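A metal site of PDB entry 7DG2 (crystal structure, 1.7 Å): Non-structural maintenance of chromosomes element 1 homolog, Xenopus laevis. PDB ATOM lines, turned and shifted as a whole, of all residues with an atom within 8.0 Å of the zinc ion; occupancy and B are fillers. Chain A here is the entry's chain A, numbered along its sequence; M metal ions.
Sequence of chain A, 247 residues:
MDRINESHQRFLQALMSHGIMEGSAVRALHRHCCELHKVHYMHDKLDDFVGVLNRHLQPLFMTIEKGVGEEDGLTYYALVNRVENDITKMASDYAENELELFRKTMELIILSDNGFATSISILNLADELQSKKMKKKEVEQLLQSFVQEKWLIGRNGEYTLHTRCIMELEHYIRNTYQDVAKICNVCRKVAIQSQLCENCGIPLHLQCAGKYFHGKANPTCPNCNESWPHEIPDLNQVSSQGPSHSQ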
ATOM      1  N   GLU A  70     -20.432 -21.873 -10.884  1.00  0.00           N
ATOM      2  CA  GLU A  70     -19.160 -21.372 -10.369  1.00  0.00           C
ATOM      3  C   GLU A  70     -18.643 -22.244  -9.240  1.00  0.00           C
ATOM      4  O   GLU A  70     -17.431 -22.470  -9.129  1.00  0.00           O
ATOM      5  CB  GLU A  70     -19.325 -19.927  -9.891  1.00  0.00           C
ATOM      6  CG  GLU A  70     -19.571 -18.974 -11.019  1.00  0.00           C
ATOM      7  CD  GLU A  70     -19.431 -17.535 -10.598  1.00  0.00           C
ATOM      8  OE1 GLU A  70     -19.529 -17.259  -9.383  1.00  0.00           O
ATOM      9  OE2 GLU A  70     -19.231 -16.677 -11.486  1.00  0.00           O
ATOM     10  N   ILE A 183     -14.600  -9.526 -14.803  1.00  0.00           N
ATOM     11  CA  ILE A 183     -14.526 -10.272 -16.059  1.00  0.00           C
ATOM     12  C   ILE A 183     -13.312 -11.198 -15.971  1.00  0.00           C
ATOM     13  O   ILE A 183     -12.170 -10.726 -15.902  1.00  0.00           O
ATOM     14  CB  ILE A 183     -14.400  -9.340 -17.270  1.00  0.00           C
ATOM     15  CG1 ILE A 183     -15.578  -8.357 -17.300  1.00  0.00           C
ATOM     16  CG2 ILE A 183     -14.346 -10.136 -18.564  1.00  0.00           C
ATOM     17  CD1 ILE A 183     -16.920  -9.024 -17.490  1.00  0.00           C
ATOM     18  N   CYS A 184     -13.566 -12.509 -15.967  1.00  0.00           N
ATOM     19  CA  CYS A 184     -12.488 -13.493 -15.785  1.00  0.00           C
ATOM     20  C   CYS A 184     -11.402 -13.296 -16.828  1.00  0.00           C
ATOM     21  O   CYS A 184     -11.676 -13.203 -18.026  1.00  0.00           O
ATOM     22  CB  CYS A 184     -13.049 -14.911 -15.878  1.00  0.00           C
ATOM     23  SG  CYS A 184     -11.793 -16.217 -15.739  1.00  0.00           S
ATOM     24  N   ASN A 185     -10.151 -13.238 -16.364  1.00  0.00           N
ATOM     25  CA  ASN A 185      -9.057 -12.953 -17.292  1.00  0.00           C
ATOM     26  C   ASN A 185      -8.820 -14.110 -18.254  1.00  0.00           C
ATOM     27  O   ASN A 185      -8.255 -13.885 -19.332  1.00  0.00           O
ATOM     28  CB  ASN A 185      -7.780 -12.611 -16.516  1.00  0.00           C
ATOM     29  CG  ASN A 185      -6.716 -11.979 -17.401  1.00  0.00           C
ATOM     30  OD1 ASN A 185      -6.843 -10.832 -17.812  1.00  0.00           O
ATOM     31  ND2 ASN A 185      -5.653 -12.741 -17.677  1.00  0.00           N
ATOM     32  N   VAL A 186      -9.271 -15.312 -17.913  1.00  0.00           N
ATOM     33  CA  VAL A 186      -9.049 -16.489 -18.749  1.00  0.00           C
ATOM     34  C   VAL A 186     -10.186 -16.704 -19.736  1.00  0.00           C
ATOM     35  O   VAL A 186      -9.958 -16.851 -20.941  1.00  0.00           O
ATOM     36  CB  VAL A 186      -8.826 -17.726 -17.853  1.00  0.00           C
ATOM     37  CG1 VAL A 186      -9.004 -19.016 -18.650  1.00  0.00           C
ATOM     38  CG2 VAL A 186      -7.455 -17.687 -17.230  1.00  0.00           C
ATOM     39  N   CYS A 187     -11.436 -16.763 -19.269  1.00  0.00           N
ATOM     40  CA  CYS A 187     -12.545 -17.073 -20.158  1.00  0.00           C
ATOM     41  C   CYS A 187     -13.328 -15.855 -20.608  1.00  0.00           C
ATOM     42  O   CYS A 187     -14.179 -15.985 -21.502  1.00  0.00           O
ATOM     43  CB  CYS A 187     -13.496 -18.076 -19.501  1.00  0.00           C
ATOM     44  SG  CYS A 187     -14.414 -17.398 -18.095  1.00  0.00           S
ATOM     45  N   ARG A 188     -13.089 -14.682 -20.004  1.00  0.00           N
ATOM     46  CA  ARG A 188     -13.700 -13.405 -20.377  1.00  0.00           C
ATOM     47  C   ARG A 188     -15.203 -13.360 -20.117  1.00  0.00           C
ATOM     48  O   ARG A 188     -15.918 -12.572 -20.739  1.00  0.00           O
ATOM     49  CB  ARG A 188     -13.399 -13.060 -21.845  1.00  0.00           C
ATOM     50  CG  ARG A 188     -11.914 -13.077 -22.193  1.00  0.00           C
ATOM     51  CD  ARG A 188     -11.181 -11.911 -21.565  1.00  0.00           C
ATOM     52  NE  ARG A 188     -11.848 -10.647 -21.845  1.00  0.00           N
ATOM     53  CZ  ARG A 188     -11.665  -9.924 -22.948  1.00  0.00           C
ATOM     54  NH1 ARG A 188     -12.331  -8.783 -23.112  1.00  0.00           N
ATOM     55  NH2 ARG A 188     -10.823 -10.345 -23.880  1.00  0.00           N
ATOM     56  N   LYS A 189     -15.706 -14.181 -19.210  1.00  0.00           N
ATOM     57  CA  LYS A 189     -17.098 -14.138 -18.787  1.00  0.00           C
ATOM     58  C   LYS A 189     -17.200 -13.551 -17.377  1.00  0.00           C
ATOM     59  O   LYS A 189     -16.228 -13.538 -16.620  1.00  0.00           O
ATOM     60  CB  LYS A 189     -17.735 -15.527 -18.824  1.00  0.00           C
ATOM     61  CG  LYS A 189     -17.731 -16.177 -20.186  1.00  0.00           C
ATOM     62  CD  LYS A 189     -18.195 -17.617 -20.113  1.00  0.00           C
ATOM     63  CE  LYS A 189     -18.414 -18.176 -21.512  1.00  0.00           C
ATOM     64  NZ  LYS A 189     -19.359 -17.305 -22.274  1.00  0.00           N
ATOM     65  N   VAL A 190     -18.400 -13.061 -17.050  1.00  0.00           N
ATOM     66  CA  VAL A 190     -18.650 -12.520 -15.716  1.00  0.00           C
ATOM     67  C   VAL A 190     -18.276 -13.551 -14.660  1.00  0.00           C
ATOM     68  O   VAL A 190     -18.586 -14.742 -14.793  1.00  0.00           O
ATOM     69  CB  VAL A 190     -20.120 -12.089 -15.572  1.00  0.00           C
ATOM     70  CG1 VAL A 190     -20.477 -11.825 -14.117  1.00  0.00           C
ATOM     71  CG2 VAL A 190     -20.394 -10.853 -16.424  1.00  0.00           C
ATOM     72  N   ALA A 191     -17.609 -13.086 -13.615  1.00  0.00           N
ATOM     73  CA  ALA A 191     -17.323 -13.910 -12.438  1.00  0.00           C
ATOM     74  C   ALA A 191     -17.948 -13.241 -11.240  1.00  0.00           C
ATOM     75  O   ALA A 191     -17.737 -12.041 -11.011  1.00  0.00           O
ATOM     76  CB  ALA A 191     -15.819 -14.095 -12.226  1.00  0.00           C
ATOM     77  N   GLN A 193     -18.174 -15.276  -7.951  1.00  0.00           N
ATOM     78  CA  GLN A 193     -17.130 -15.808  -7.092  1.00  0.00           C
ATOM     79  C   GLN A 193     -15.855 -15.972  -7.919  1.00  0.00           C
ATOM     80  O   GLN A 193     -15.903 -16.373  -9.080  1.00  0.00           O
ATOM     81  CB  GLN A 193     -17.540 -17.149  -6.487  1.00  0.00           C
ATOM     82  CG  GLN A 193     -18.785 -17.046  -5.614  1.00  0.00           C
ATOM     83  CD  GLN A 193     -19.139 -18.362  -4.971  1.00  0.00           C
ATOM     84  OE1 GLN A 193     -20.180 -18.959  -5.263  1.00  0.00           O
ATOM     85  NE2 GLN A 193     -18.287 -18.815  -4.052  1.00  0.00           N
ATOM     86  N   PRO A 203      -9.574 -10.738 -11.842  1.00  0.00           N
ATOM     87  CA  PRO A 203     -10.249 -11.923 -11.314  1.00  0.00           C
ATOM     88  C   PRO A 203     -10.069 -13.148 -12.207  1.00  0.00           C
ATOM     89  O   PRO A 203      -9.933 -13.020 -13.429  1.00  0.00           O
ATOM     90  CB  PRO A 203     -11.716 -11.483 -11.284  1.00  0.00           C
ATOM     91  CG  PRO A 203     -11.835 -10.603 -12.513  1.00  0.00           C
ATOM     92  CD  PRO A 203     -10.468  -9.946 -12.719  1.00  0.00           C
ATOM     93  N   LEU A 204     -10.078 -14.336 -11.600  1.00  0.00           N
ATOM     94  CA  LEU A 204     -10.237 -15.583 -12.318  1.00  0.00           C
ATOM     95  C   LEU A 204     -11.342 -16.395 -11.656  1.00  0.00           C
ATOM     96  O   LEU A 204     -11.431 -16.418 -10.425  1.00  0.00           O
ATOM     97  CB  LEU A 204      -8.940 -16.411 -12.330  1.00  0.00           C
ATOM     98  CG  LEU A 204      -7.793 -15.931 -13.213  1.00  0.00           C
ATOM     99  CD1 LEU A 204      -6.759 -17.041 -13.374  1.00  0.00           C
ATOM    100  CD2 LEU A 204      -8.325 -15.492 -14.564  1.00  0.00           C
ATOM    101  N   HIS A 205     -12.178 -17.054 -12.457  1.00  0.00           N
ATOM    102  CA  HIS A 205     -13.059 -18.071 -11.897  1.00  0.00           C
ATOM    103  C   HIS A 205     -12.229 -19.126 -11.170  1.00  0.00           C
ATOM    104  O   HIS A 205     -11.089 -19.410 -11.548  1.00  0.00           O
ATOM    105  CB  HIS A 205     -13.876 -18.773 -12.986  1.00  0.00           C
ATOM    106  CG  HIS A 205     -14.964 -17.941 -13.586  1.00  0.00           C
ATOM    107  ND1 HIS A 205     -14.939 -17.523 -14.894  1.00  0.00           N
ATOM    108  CD2 HIS A 205     -16.117 -17.460 -13.054  1.00  0.00           C
ATOM    109  CE1 HIS A 205     -16.028 -16.821 -15.158  1.00  0.00           C
ATOM    110  NE2 HIS A 205     -16.752 -16.757 -14.058  1.00  0.00           N
ATOM    111  N   LEU A 206     -12.812 -19.715 -10.130  1.00  0.00           N
ATOM    112  CA  LEU A 206     -12.095 -20.744  -9.382  1.00  0.00           C
ATOM    113  C   LEU A 206     -11.743 -21.929 -10.287  1.00  0.00           C
ATOM    114  O   LEU A 206     -10.630 -22.459 -10.203  1.00  0.00           O
ATOM    115  CB  LEU A 206     -12.913 -21.202  -8.180  1.00  0.00           C
ATOM    116  CG  LEU A 206     -12.420 -20.618  -6.846  1.00  0.00           C
ATOM    117  CD1 LEU A 206     -12.718 -19.131  -6.767  1.00  0.00           C
ATOM    118  CD2 LEU A 206     -13.009 -21.365  -5.646  1.00  0.00           C
ATOM    119  N   GLN A 207     -12.664 -22.333 -11.159  1.00  0.00           N
ATOM    120  CA  GLN A 207     -12.358 -23.398 -12.101  1.00  0.00           C
ATOM    121  C   GLN A 207     -11.319 -22.954 -13.124  1.00  0.00           C
ATOM    122  O   GLN A 207     -10.489 -23.759 -13.553  1.00  0.00           O
ATOM    123  CB  GLN A 207     -13.624 -23.871 -12.820  1.00  0.00           C
ATOM    124  CG  GLN A 207     -14.210 -25.162 -12.268  1.00  0.00           C
ATOM    125  CD  GLN A 207     -15.366 -24.908 -11.314  1.00  0.00           C
ATOM    126  OE1 GLN A 207     -16.300 -24.158 -11.616  1.00  0.00           O
ATOM    127  NE2 GLN A 207     -15.304 -25.543 -10.137  1.00  0.00           N
ATOM    128  N   CYS A 208     -11.346 -21.683 -13.523  1.00  0.00           N
ATOM    129  CA  CYS A 208     -10.361 -21.220 -14.492  1.00  0.00           C
ATOM    130  C   CYS A 208      -8.984 -21.071 -13.878  1.00  0.00           C
ATOM    131  O   CYS A 208      -7.981 -21.272 -14.570  1.00  0.00           O
ATOM    132  CB  CYS A 208     -10.826 -19.899 -15.110  1.00  0.00           C
ATOM    133  SG  CYS A 208     -12.340 -20.059 -16.088  1.00  0.00           S
ATOM    134  N   ALA A 209      -8.903 -20.732 -12.591  1.00  0.00           N
ATOM    135  CA  ALA A 209      -7.602 -20.706 -11.918  1.00  0.00           C
ATOM    136  C   ALA A 209      -6.998 -22.109 -11.839  1.00  0.00           C
ATOM    137  O   ALA A 209      -5.792 -22.282 -12.049  1.00  0.00           O
ATOM    138  CB  ALA A 209      -7.737 -20.100 -10.525  1.00  0.00           C
ATOM    139  N   LYS A 211      -7.436 -24.566 -13.926  1.00  0.00           N
ATOM    140  CA  LYS A 211      -6.940 -24.938 -15.252  1.00  0.00           C
ATOM    141  C   LYS A 211      -5.677 -24.161 -15.608  1.00  0.00           C
ATOM    142  O   LYS A 211      -4.650 -24.741 -15.975  1.00  0.00           O
ATOM    143  CB  LYS A 211      -8.029 -24.700 -16.294  1.00  0.00           C
ATOM    144  CG  LYS A 211      -9.154 -25.733 -16.277  1.00  0.00           C
ATOM    145  CD  LYS A 211     -10.348 -25.256 -17.099  1.00  0.00           C
ATOM    146  CE  LYS A 211      -9.917 -24.775 -18.476  1.00  0.00           C
ATOM    147  NZ  LYS A 211     -11.076 -24.209 -19.234  1.00  0.00           N
HETATM  148 ZN    ZN M   1     -13.318 -17.916 -16.232  1.00  0.00          ZN
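N of Val 186 sits close to SG of Cys 184, at 3.5 Å. SG of Cys 187 sits close to N of Lys 189 (3.6 Å). N of Cys 184 lies within hydrogen-bond range of O of Lys 189, 2.9 Å away. NE2 of His 205 lies within hydrogen-bond range of O of Val 190.
Along chain A the residues within 4 Å of the zinc ion span positions 184 to 208. The nearest printed residue that does not touch the zinc ion is Val 186 (4.8 Å).
The zinc ion is bound by ND1 of His 205 (2.1 Å), SG of Cys 187 (2.2 Å), SG of Cys 184 (2.3 Å) and SG of Cys 208 (2.4 Å). The zinc ion has four donor atoms within binding distance.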
